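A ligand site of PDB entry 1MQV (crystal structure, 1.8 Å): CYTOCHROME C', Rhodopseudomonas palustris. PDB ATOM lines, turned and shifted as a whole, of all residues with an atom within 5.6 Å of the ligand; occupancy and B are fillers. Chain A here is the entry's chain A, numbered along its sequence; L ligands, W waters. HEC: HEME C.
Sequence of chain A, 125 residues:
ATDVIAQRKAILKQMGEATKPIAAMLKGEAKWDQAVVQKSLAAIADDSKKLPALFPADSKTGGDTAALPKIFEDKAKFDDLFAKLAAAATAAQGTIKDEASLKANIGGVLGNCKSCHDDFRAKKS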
ATOM      1  N   ILE A   5       7.871   6.807 -20.984  1.00  0.00           N
ATOM      2  CA  ILE A   5       9.319   6.610 -21.097  1.00  0.00           C
ATOM      3  C   ILE A   5       9.926   7.984 -21.291  1.00  0.00           C
ATOM      4  O   ILE A   5      10.961   8.300 -20.729  1.00  0.00           O
ATOM      5  CB  ILE A   5       9.708   5.663 -22.287  1.00  0.00           C
ATOM      6  CG1 ILE A   5       9.532   4.210 -21.849  1.00  0.00           C
ATOM      7  CG2 ILE A   5      11.186   5.795 -22.682  1.00  0.00           C
ATOM      8  CD1 ILE A   5       9.564   3.225 -22.997  1.00  0.00           C
ATOM      9  N   ARG A   8       9.631   9.885 -17.768  1.00  0.00           N
ATOM     10  CA  ARG A   8      10.576   9.453 -16.715  1.00  0.00           C
ATOM     11  C   ARG A   8      12.009   9.787 -17.069  1.00  0.00           C
ATOM     12  O   ARG A   8      12.786  10.138 -16.189  1.00  0.00           O
ATOM     13  CB  ARG A   8      10.397   7.941 -16.412  1.00  0.00           C
ATOM     14  CG  ARG A   8      10.911   6.986 -17.497  1.00  0.00           C
ATOM     15  CD  ARG A   8      10.163   5.682 -17.441  1.00  0.00           C
ATOM     16  NE  ARG A   8      10.827   4.619 -18.189  1.00  0.00           N
ATOM     17  CZ  ARG A   8      10.264   3.442 -18.470  1.00  0.00           C
ATOM     18  NH1 ARG A   8       9.015   3.179 -18.083  1.00  0.00           N
ATOM     19  NH2 ARG A   8      10.941   2.517 -19.139  1.00  0.00           N
ATOM     20  N   LYS A   9      12.379   9.744 -18.351  1.00  0.00           N
ATOM     21  CA  LYS A   9      13.748  10.096 -18.696  1.00  0.00           C
ATOM     22  C   LYS A   9      13.995  11.576 -18.444  1.00  0.00           C
ATOM     23  O   LYS A   9      15.122  11.981 -18.099  1.00  0.00           O
ATOM     24  CB  LYS A   9      14.022   9.748 -20.171  1.00  0.00           C
ATOM     25  CG  LYS A   9      14.397   8.271 -20.449  1.00  0.00           C
ATOM     26  CD  LYS A   9      14.527   8.107 -21.983  1.00  0.00           C
ATOM     27  CE  LYS A   9      15.605   7.158 -22.400  1.00  0.00           C
ATOM     28  NZ  LYS A   9      15.672   7.182 -23.892  1.00  0.00           N
ATOM     29  N   LEU A  12      14.515  11.917 -14.684  1.00  0.00           N
ATOM     30  CA  LEU A  12      15.814  11.374 -14.249  1.00  0.00           C
ATOM     31  C   LEU A  12      16.932  12.240 -14.777  1.00  0.00           C
ATOM     32  O   LEU A  12      17.982  12.357 -14.140  1.00  0.00           O
ATOM     33  CB  LEU A  12      15.983   9.907 -14.703  1.00  0.00           C
ATOM     34  CG  LEU A  12      15.023   8.952 -14.009  1.00  0.00           C
ATOM     35  CD1 LEU A  12      14.761   7.734 -14.886  1.00  0.00           C
ATOM     36  CD2 LEU A  12      15.690   8.508 -12.619  1.00  0.00           C
ATOM     37  N   LYS A  13      16.735  12.877 -15.927  1.00  0.00           N
ATOM     38  CA  LYS A  13      17.763  13.788 -16.451  1.00  0.00           C
ATOM     39  C   LYS A  13      17.884  14.949 -15.470  1.00  0.00           C
ATOM     40  O   LYS A  13      19.012  15.388 -15.152  1.00  0.00           O
ATOM     41  CB  LYS A  13      17.380  14.285 -17.862  1.00  0.00           C
ATOM     42  CG  LYS A  13      18.343  15.291 -18.441  1.00  0.00           C
ATOM     43  CD  LYS A  13      18.025  15.511 -19.932  1.00  0.00           C
ATOM     44  CE  LYS A  13      18.744  16.727 -20.495  1.00  0.00           C
ATOM     45  NZ  LYS A  13      20.201  16.735 -20.180  1.00  0.00           N
ATOM     46  N   MET A  15      17.229  14.821 -12.317  1.00  0.00           N
ATOM     47  CA  MET A  15      17.888  14.321 -11.102  1.00  0.00           C
ATOM     48  C   MET A  15      19.392  14.359 -11.326  1.00  0.00           C
ATOM     49  O   MET A  15      20.150  14.809 -10.446  1.00  0.00           O
ATOM     50  CB  MET A  15      17.432  12.888 -10.759  1.00  0.00           C
ATOM     51  CG  MET A  15      16.216  12.787  -9.878  1.00  0.00           C
ATOM     52  SD  MET A  15      16.450  11.621  -8.469  1.00  0.00           S
ATOM     53  CE  MET A  15      15.954  10.187  -9.242  1.00  0.00           C
ATOM     54  N   GLY A  16      19.830  13.910 -12.505  1.00  0.00           N
ATOM     55  CA  GLY A  16      21.251  13.953 -12.829  1.00  0.00           C
ATOM     56  C   GLY A  16      21.798  15.380 -12.729  1.00  0.00           C
ATOM     57  O   GLY A  16      22.865  15.615 -12.116  1.00  0.00           O
ATOM     58  N   THR A  19      22.522  16.744  -9.251  1.00  0.00           N
ATOM     59  CA  THR A  19      23.739  16.294  -8.556  1.00  0.00           C
ATOM     60  C   THR A  19      24.964  17.061  -9.024  1.00  0.00           C
ATOM     61  O   THR A  19      25.978  17.076  -8.341  1.00  0.00           O
ATOM     62  CB  THR A  19      24.053  14.765  -8.730  1.00  0.00           C
ATOM     63  OG1 THR A  19      24.411  14.514 -10.107  1.00  0.00           O
ATOM     64  CG2 THR A  19      22.875  13.913  -8.355  1.00  0.00           C
ATOM     65  N   ILE A  44      15.741  16.042  -5.918  1.00  0.00           N
ATOM     66  CA  ILE A  44      15.953  14.594  -5.851  1.00  0.00           C
ATOM     67  C   ILE A  44      14.772  13.962  -5.115  1.00  0.00           C
ATOM     68  O   ILE A  44      14.205  12.966  -5.584  1.00  0.00           O
ATOM     69  CB  ILE A  44      17.331  14.265  -5.157  1.00  0.00           C
ATOM     70  CG1 ILE A  44      18.475  14.663  -6.077  1.00  0.00           C
ATOM     71  CG2 ILE A  44      17.423  12.757  -4.806  1.00  0.00           C
ATOM     72  CD1 ILE A  44      19.860  14.690  -5.357  1.00  0.00           C
ATOM     73  N   PHE A  55       6.656   3.530 -14.420  1.00  0.00           N
ATOM     74  CA  PHE A  55       7.257   2.324 -14.969  1.00  0.00           C
ATOM     75  C   PHE A  55       6.213   1.211 -15.125  1.00  0.00           C
ATOM     76  O   PHE A  55       6.245   0.202 -14.447  1.00  0.00           O
ATOM     77  CB  PHE A  55       8.432   1.827 -14.080  1.00  0.00           C
ATOM     78  CG  PHE A  55       9.659   2.708 -14.146  1.00  0.00           C
ATOM     79  CD1 PHE A  55       9.733   3.882 -13.380  1.00  0.00           C
ATOM     80  CD2 PHE A  55      10.706   2.410 -15.016  1.00  0.00           C
ATOM     81  CE1 PHE A  55      10.819   4.731 -13.481  1.00  0.00           C
ATOM     82  CE2 PHE A  55      11.820   3.266 -15.130  1.00  0.00           C
ATOM     83  CZ  PHE A  55      11.867   4.433 -14.351  1.00  0.00           C
ATOM     84  N   ASP A  64      12.856   2.811 -26.578  1.00  0.00           N
ATOM     85  CA  ASP A  64      13.883   3.823 -26.367  1.00  0.00           C
ATOM     86  C   ASP A  64      14.124   4.007 -24.878  1.00  0.00           C
ATOM     87  O   ASP A  64      14.122   5.145 -24.398  1.00  0.00           O
ATOM     88  CB  ASP A  64      13.430   5.148 -26.980  1.00  0.00           C
ATOM     89  CG  ASP A  64      12.043   5.555 -26.494  1.00  0.00           C
ATOM     90  OD1 ASP A  64      11.448   4.779 -25.711  1.00  0.00           O
ATOM     91  OD2 ASP A  64      11.557   6.639 -26.889  1.00  0.00           O
ATOM     92  N   THR A  65      14.301   2.907 -24.153  1.00  0.00           N
ATOM     93  CA  THR A  65      14.479   3.014 -22.712  1.00  0.00           C
ATOM     94  C   THR A  65      15.628   2.154 -22.232  1.00  0.00           C
ATOM     95  O   THR A  65      15.944   1.125 -22.823  1.00  0.00           O
ATOM     96  CB  THR A  65      13.204   2.549 -21.983  1.00  0.00           C
ATOM     97  OG1 THR A  65      13.455   2.477 -20.565  1.00  0.00           O
ATOM     98  CG2 THR A  65      12.821   1.126 -22.446  1.00  0.00           C
ATOM     99  N   ALA A  66      16.261   2.571 -21.147  1.00  0.00           N
ATOM    100  CA  ALA A  66      17.359   1.798 -20.604  1.00  0.00           C
ATOM    101  C   ALA A  66      16.875   1.010 -19.390  1.00  0.00           C
ATOM    102  O   ALA A  66      17.660   0.401 -18.705  1.00  0.00           O
ATOM    103  CB  ALA A  66      18.517   2.714 -20.214  1.00  0.00           C
ATOM    104  N   ALA A  67      15.583   1.076 -19.104  1.00  0.00           N
ATOM    105  CA  ALA A  67      15.031   0.316 -17.991  1.00  0.00           C
ATOM    106  C   ALA A  67      15.093  -1.170 -18.333  1.00  0.00           C
ATOM    107  O   ALA A  67      14.697  -1.587 -19.406  1.00  0.00           O
ATOM    108  CB  ALA A  67      13.614   0.732 -17.765  1.00  0.00           C
ATOM    109  N   LEU A  68      15.596  -1.977 -17.395  1.00  0.00           N
ATOM    110  CA  LEU A  68      15.712  -3.414 -17.628  1.00  0.00           C
ATOM    111  C   LEU A  68      14.429  -4.159 -17.282  1.00  0.00           C
ATOM    112  O   LEU A  68      13.685  -3.778 -16.394  1.00  0.00           O
ATOM    113  CB  LEU A  68      16.895  -3.994 -16.817  1.00  0.00           C
ATOM    114  CG  LEU A  68      18.271  -3.379 -17.113  1.00  0.00           C
ATOM    115  CD1 LEU A  68      19.329  -3.984 -16.178  1.00  0.00           C
ATOM    116  CD2 LEU A  68      18.637  -3.628 -18.602  1.00  0.00           C
ATOM    117  N   ILE A  71      13.002  -5.108 -13.640  1.00  0.00           N
ATOM    118  CA  ILE A  71      12.145  -4.247 -12.853  1.00  0.00           C
ATOM    119  C   ILE A  71      10.795  -4.888 -12.552  1.00  0.00           C
ATOM    120  O   ILE A  71      10.308  -4.851 -11.418  1.00  0.00           O
ATOM    121  CB  ILE A  71      11.894  -2.933 -13.603  1.00  0.00           C
ATOM    122  CG1 ILE A  71      13.225  -2.158 -13.649  1.00  0.00           C
ATOM    123  CG2 ILE A  71      10.699  -2.160 -12.962  1.00  0.00           C
ATOM    124  CD1 ILE A  71      13.226  -0.925 -14.567  1.00  0.00           C
ATOM    125  N   PHE A  78      12.053  -2.363  -6.476  1.00  0.00           N
ATOM    126  CA  PHE A  78      12.376  -1.213  -7.309  1.00  0.00           C
ATOM    127  C   PHE A  78      11.657   0.023  -6.764  1.00  0.00           C
ATOM    128  O   PHE A  78      12.315   1.049  -6.536  1.00  0.00           O
ATOM    129  CB  PHE A  78      11.979  -1.529  -8.779  1.00  0.00           C
ATOM    130  CG  PHE A  78      12.080  -0.357  -9.735  1.00  0.00           C
ATOM    131  CD1 PHE A  78      13.314  -0.034 -10.338  1.00  0.00           C
ATOM    132  CD2 PHE A  78      10.943   0.342 -10.107  1.00  0.00           C
ATOM    133  CE1 PHE A  78      13.376   0.960 -11.312  1.00  0.00           C
ATOM    134  CE2 PHE A  78      11.002   1.347 -11.090  1.00  0.00           C
ATOM    135  CZ  PHE A  78      12.231   1.647 -11.685  1.00  0.00           C
ATOM    136  N   LEU A  81      13.157   1.444  -3.580  1.00  0.00           N
ATOM    137  CA  LEU A  81      14.484   2.051  -3.678  1.00  0.00           C
ATOM    138  C   LEU A  81      14.240   3.518  -4.003  1.00  0.00           C
ATOM    139  O   LEU A  81      15.026   4.381  -3.641  1.00  0.00           O
ATOM    140  CB  LEU A  81      15.341   1.384  -4.784  1.00  0.00           C
ATOM    141  CG  LEU A  81      16.818   1.060  -4.486  1.00  0.00           C
ATOM    142  CD1 LEU A  81      17.480   2.209  -3.724  1.00  0.00           C
ATOM    143  CD2 LEU A  81      16.858  -0.219  -3.637  1.00  0.00           C
ATOM    144  N   PHE A  82      13.157   3.833  -4.734  1.00  0.00           N
ATOM    145  CA  PHE A  82      12.931   5.246  -4.984  1.00  0.00           C
ATOM    146  C   PHE A  82      12.455   5.868  -3.666  1.00  0.00           C
ATOM    147  O   PHE A  82      12.770   7.018  -3.357  1.00  0.00           O
ATOM    148  CB  PHE A  82      11.858   5.491  -6.036  1.00  0.00           C
ATOM    149  CG  PHE A  82      12.362   5.432  -7.426  1.00  0.00           C
ATOM    150  CD1 PHE A  82      13.304   6.350  -7.878  1.00  0.00           C
ATOM    151  CD2 PHE A  82      11.836   4.515  -8.319  1.00  0.00           C
ATOM    152  CE1 PHE A  82      13.709   6.368  -9.200  1.00  0.00           C
ATOM    153  CE2 PHE A  82      12.230   4.532  -9.650  1.00  0.00           C
ATOM    154  CZ  PHE A  82      13.161   5.457 -10.090  1.00  0.00           C
ATOM    155  N   LEU A  85      15.469   6.617  -1.670  1.00  0.00           N
ATOM    156  CA  LEU A  85      16.171   7.804  -2.072  1.00  0.00           C
ATOM    157  C   LEU A  85      15.413   9.056  -1.662  1.00  0.00           C
ATOM    158  O   LEU A  85      16.008  10.033  -1.258  1.00  0.00           O
ATOM    159  CB  LEU A  85      16.429   7.774  -3.601  1.00  0.00           C
ATOM    160  CG  LEU A  85      17.018   9.062  -4.204  1.00  0.00           C
ATOM    161  CD1 LEU A  85      18.434   9.452  -3.582  1.00  0.00           C
ATOM    162  CD2 LEU A  85      17.120   8.780  -5.723  1.00  0.00           C
ATOM    163  N   VAL A 109      22.971   9.579   0.382  1.00  0.00           N
ATOM    164  CA  VAL A 109      22.001   9.951  -0.622  1.00  0.00           C
ATOM    165  C   VAL A 109      22.383   9.376  -1.975  1.00  0.00           C
ATOM    166  O   VAL A 109      21.617   8.583  -2.597  1.00  0.00           O
ATOM    167  CB  VAL A 109      21.928  11.492  -0.750  1.00  0.00           C
ATOM    168  CG1 VAL A 109      20.863  11.877  -1.761  1.00  0.00           C
ATOM    169  CG2 VAL A 109      21.622  12.118   0.638  1.00  0.00           C
ATOM    170  N   LEU A 110      23.565   9.778  -2.445  1.00  0.00           N
ATOM    171  CA  LEU A 110      24.054   9.370  -3.749  1.00  0.00           C
ATOM    172  C   LEU A 110      24.293   7.893  -3.960  1.00  0.00           C
ATOM    173  O   LEU A 110      24.299   7.422  -5.097  1.00  0.00           O
ATOM    174  CB  LEU A 110      25.326  10.166  -4.109  1.00  0.00           C
ATOM    175  CG  LEU A 110      25.270  11.714  -4.067  1.00  0.00           C
ATOM    176  CD1 LEU A 110      26.554  12.277  -4.639  1.00  0.00           C
ATOM    177  CD2 LEU A 110      24.060  12.209  -4.901  1.00  0.00           C
ATOM    178  N   ASN A 112      22.335   5.562  -3.468  1.00  0.00           N
ATOM    179  CA  ASN A 112      21.105   4.986  -3.924  1.00  0.00           C
ATOM    180  C   ASN A 112      21.069   4.995  -5.455  1.00  0.00           C
ATOM    181  O   ASN A 112      20.435   4.121  -6.038  1.00  0.00           O
ATOM    182  CB  ASN A 112      19.924   5.801  -3.374  1.00  0.00           C
ATOM    183  CG  ASN A 112      19.686   5.515  -1.931  1.00  0.00           C
ATOM    184  OD1 ASN A 112      19.338   4.377  -1.579  1.00  0.00           O
ATOM    185  ND2 ASN A 112      19.896   6.520  -1.063  1.00  0.00           N
ATOM    186  N   CYS A 113      21.745   5.966  -6.093  1.00  0.00           N
ATOM    187  CA  CYS A 113      21.717   6.022  -7.560  1.00  0.00           C
ATOM    188  C   CYS A 113      22.332   4.728  -8.127  1.00  0.00           C
ATOM    189  O   CYS A 113      21.669   3.975  -8.859  1.00  0.00           O
ATOM    190  CB  CYS A 113      22.500   7.246  -8.091  1.00  0.00           C
ATOM    191  SG  CYS A 113      22.107   8.818  -7.247  1.00  0.00           S
ATOM    192  N   CYS A 116      20.449   1.241  -7.569  1.00  0.00           N
ATOM    193  CA  CYS A 116      19.360   0.882  -8.421  1.00  0.00           C
ATOM    194  C   CYS A 116      19.899   0.626  -9.831  1.00  0.00           C
ATOM    195  O   CYS A 116      19.499  -0.331 -10.490  1.00  0.00           O
ATOM    196  CB  CYS A 116      18.346   2.022  -8.483  1.00  0.00           C
ATOM    197  SG  CYS A 116      16.995   1.592  -9.510  1.00  0.00           S
ATOM    198  N   HIS A 117      20.800   1.487 -10.292  1.00  0.00           N
ATOM    199  CA  HIS A 117      21.342   1.309 -11.646  1.00  0.00           C
ATOM    200  C   HIS A 117      21.975  -0.070 -11.827  1.00  0.00           C
ATOM    201  O   HIS A 117      21.769  -0.702 -12.850  1.00  0.00           O
ATOM    202  CB  HIS A 117      22.348   2.441 -11.978  1.00  0.00           C
ATOM    203  CG  HIS A 117      21.714   3.802 -12.030  1.00  0.00           C
ATOM    204  ND1 HIS A 117      22.434   4.964 -11.931  1.00  0.00           N
ATOM    205  CD2 HIS A 117      20.419   4.173 -12.166  1.00  0.00           C
ATOM    206  CE1 HIS A 117      21.622   5.999 -12.016  1.00  0.00           C
ATOM    207  NE2 HIS A 117      20.383   5.544 -12.159  1.00  0.00           N
ATOM    208  N   PHE A 120      18.756  -2.412 -12.302  1.00  0.00           N
ATOM    209  CA  PHE A 120      17.617  -2.086 -13.157  1.00  0.00           C
ATOM    210  C   PHE A 120      17.829  -1.146 -14.345  1.00  0.00           C
ATOM    211  O   PHE A 120      16.841  -0.801 -15.005  1.00  0.00           O
ATOM    212  CB  PHE A 120      16.556  -1.478 -12.242  1.00  0.00           C
ATOM    213  CG  PHE A 120      16.160  -2.387 -11.089  1.00  0.00           C
ATOM    214  CD1 PHE A 120      15.478  -3.568 -11.336  1.00  0.00           C
ATOM    215  CD2 PHE A 120      16.469  -2.062  -9.759  1.00  0.00           C
ATOM    216  CE1 PHE A 120      15.081  -4.417 -10.279  1.00  0.00           C
ATOM    217  CE2 PHE A 120      16.078  -2.898  -8.712  1.00  0.00           C
ATOM    218  CZ  PHE A 120      15.375  -4.083  -8.967  1.00  0.00           C
ATOM    219  N   ARG A 121      19.078  -0.752 -14.602  1.00  0.00           N
ATOM    220  CA  ARG A 121      19.409   0.150 -15.707  1.00  0.00           C
ATOM    221  C   ARG A 121      20.431  -0.483 -16.639  1.00  0.00           C
ATOM    222  O   ARG A 121      21.352  -1.136 -16.195  1.00  0.00           O
ATOM    223  CB  ARG A 121      19.951   1.472 -15.180  1.00  0.00           C
ATOM    224  CG  ARG A 121      20.171   2.545 -16.248  1.00  0.00           C
ATOM    225  CD  ARG A 121      21.050   3.680 -15.686  1.00  0.00           C
ATOM    226  NE  ARG A 121      21.320   4.694 -16.684  1.00  0.00           N
ATOM    227  CZ  ARG A 121      21.719   5.932 -16.398  1.00  0.00           C
ATOM    228  NH1 ARG A 121      21.881   6.288 -15.138  1.00  0.00           N
ATOM    229  NH2 ARG A 121      21.957   6.805 -17.373  1.00  0.00           N
HETATM  230 FE   HEC L   1      18.687   6.773 -12.413  1.00  0.00          FE
HETATM  231  CHA HEC L   1      18.173   6.750 -15.746  1.00  0.00           C
HETATM  232  CHB HEC L   1      20.404   9.716 -12.718  1.00  0.00           C
HETATM  233  CHC HEC L   1      18.557   7.230  -9.059  1.00  0.00           C
HETATM  234  CHD HEC L   1      16.536   3.999 -12.021  1.00  0.00           C
HETATM  235  NA  HEC L   1      19.211   8.010 -13.972  1.00  0.00           N
HETATM  236  C1A HEC L   1      18.874   7.800 -15.269  1.00  0.00           C
HETATM  237  C2A HEC L   1      19.406   8.850 -16.055  1.00  0.00           C
HETATM  238  C3A HEC L   1      20.098   9.730 -15.216  1.00  0.00           C
HETATM  239  C4A HEC L   1      19.941   9.165 -13.895  1.00  0.00           C
HETATM  240  CMA HEC L   1      20.889  10.978 -15.442  1.00  0.00           C
HETATM  241  CAA HEC L   1      19.325   8.942 -17.574  1.00  0.00           C
HETATM  242  CBA HEC L   1      18.065   9.682 -17.968  1.00  0.00           C
HETATM  243  CGA HEC L   1      18.027   9.984 -19.467  1.00  0.00           C
HETATM  244  O1A HEC L   1      18.332  11.127 -19.833  1.00  0.00           O
HETATM  245  O2A HEC L   1      17.706   9.074 -20.253  1.00  0.00           O
HETATM  246  NB  HEC L   1      19.349   8.132 -11.191  1.00  0.00           N
HETATM  247  C1B HEC L   1      20.156   9.231 -11.441  1.00  0.00           C
HETATM  248  C2B HEC L   1      20.659   9.876 -10.212  1.00  0.00           C
HETATM  249  C3B HEC L   1      20.157   9.175  -9.192  1.00  0.00           C
HETATM  250  C4B HEC L   1      19.300   8.110  -9.802  1.00  0.00           C
HETATM  251  CMB HEC L   1      21.632  11.103 -10.210  1.00  0.00           C
HETATM  252  CAB HEC L   1      20.359   9.368  -7.758  1.00  0.00           C
HETATM  253  CBB HEC L   1      20.223  10.608  -7.112  1.00  0.00           C
HETATM  254  NC  HEC L   1      17.693   5.875 -10.902  1.00  0.00           N
HETATM  255  C1C HEC L   1      17.773   6.176  -9.546  1.00  0.00           C
HETATM  256  C2C HEC L   1      17.077   5.238  -8.752  1.00  0.00           C
HETATM  257  C3C HEC L   1      16.507   4.284  -9.551  1.00  0.00           C
HETATM  258  C4C HEC L   1      16.928   4.718 -10.925  1.00  0.00           C
HETATM  259  CMC HEC L   1      17.127   5.177  -7.186  1.00  0.00           C
HETATM  260  CAC HEC L   1      15.756   3.061  -9.287  1.00  0.00           C
HETATM  261  CBC HEC L   1      15.045   2.961  -8.004  1.00  0.00           C
HETATM  262  ND  HEC L   1      17.559   5.563 -13.607  1.00  0.00           N
HETATM  263  C1D HEC L   1      16.843   4.418 -13.351  1.00  0.00           C
HETATM  264  C2D HEC L   1      16.401   3.766 -14.599  1.00  0.00           C
HETATM  265  C3D HEC L   1      16.876   4.562 -15.608  1.00  0.00           C
HETATM  266  C4D HEC L   1      17.585   5.693 -15.005  1.00  0.00           C
HETATM  267  CMD HEC L   1      15.353   2.607 -14.596  1.00  0.00           C
HETATM  268  CAD HEC L   1      16.580   4.303 -17.167  1.00  0.00           C
HETATM  269  CBD HEC L   1      15.324   5.187 -17.461  1.00  0.00           C
HETATM  270  CGD HEC L   1      14.791   4.879 -18.853  1.00  0.00           C
HETATM  271  O1D HEC L   1      15.650   4.804 -19.742  1.00  0.00           O
HETATM  272  O2D HEC L   1      13.566   4.705 -19.027  1.00  0.00           O
HETATM  273  O   HOH W   1      18.603   8.923 -22.700  1.00  0.00           O
HETATM  274  O   HOH W   2      17.191  12.307 -22.018  1.00  0.00           O
HETATM  275  O   HOH W   3      20.701  12.752 -18.924  1.00  0.00           O
HETATM  276  O   HOH W   4      17.826   6.476 -19.765  1.00  0.00           O
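The backbone carbonyl oxygen (O) of Phe 120 is in hydrogen-bond range of the backbone NH (N) of Leu 68 (2.9 Å). The side-chain hydroxyl (OG1) of Thr 65 sits at hydrogen-bond distance from the backbone NH (N) of Ala 67, at 2.9 Å. The side-chain amino group (NZ) of Lys 9 lies within hydrogen-bond range of the backbone carbonyl oxygen (O) of Asp 64 (2.6 Å). The side-chain hydroxyl (OG1) of Thr 65 is in hydrogen-bond range of the guanidinium group (NH2) of Arg 8 (2.9 Å). The side-chain hydroxyl of Thr 19 lies within hydrogen-bond range of the backbone carbonyl oxygen of Gly 16. O of Cys 113 lies close to ND1 of His 117 (3.3 Å). A ring nitrogen (NE2) of His 117 lies close to the guanidinium group (NH1) of Arg 121, 3.4 Å away. The side-chain amide nitrogen (ND2) of Asn 112 sits at hydrogen-bond distance from the backbone carbonyl oxygen (O) of Val 109, 3.1 Å away.
A ring nitrogen (NE2) of His 117 is bound to an iron atom (FE) of the ligand. The side-chain sulfur of Cys 113 is covalently linked to a carbon (CAB) of the ligand (1.9 Å). O2D of the ligand is in salt-bridge range of NE of Arg 8 (2.9 Å). OG1 of Thr 65 sits at hydrogen-bond distance from O2D of the ligand (2.7 Å). The backbone NH of Ala 66 lies within hydrogen-bond range of an oxygen (O1D) of the ligand (2.7 Å). CAC of the ligand is bonded to SG of Cys 116 (1.9 Å).
A nitrogen (NA) of the ligand lies close to the guanidinium group of Arg 121 (3.4 Å). Lys 9 touches the ligand. Leu 12 touches the ligand. Lys 13 touches the ligand (CB to O1A, 3.8 Å). Met 15 touches the ligand. CA of Gly 16 touches CMB of the ligand, at 3.9 Å. Thr 19 touches the ligand. CE2 of Phe 55 touches CMD of the ligand (3.6 Å). Ala 67 touches the ligand. O of Phe 78 touches CBC of the ligand (3.6 Å). Leu 81 touches the ligand. Phe 82 touches the ligand (CE1 to C3C, 3.5 Å). CD2 of Leu 85 touches CBB of the ligand, 3.9 Å away. O of Asn 112 touches CMC of the ligand (3.7 Å). Phe 120 touches the ligand. Hydrophobic or aromatic side chains within 4 Å of the ligand: Leu 12, Met 15, Phe 55, Ala 66, Phe 78, Leu 81, Phe 82, Leu 85 and His 117. Within 4 Å of the ligand: Arg 8, Lys 9, Leu 12, Lys 13, Met 15, Gly 16, Thr 19, Phe 55, Thr 65, Ala 66, Ala 67, Phe 78, Leu 81, Phe 82, Leu 85, Asn 112, Cys 113, Cys 116, His 117, Phe 120 and Arg 121. The nearest printed residue that does not touch the ligand is Ile 71 (4.1 Å).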
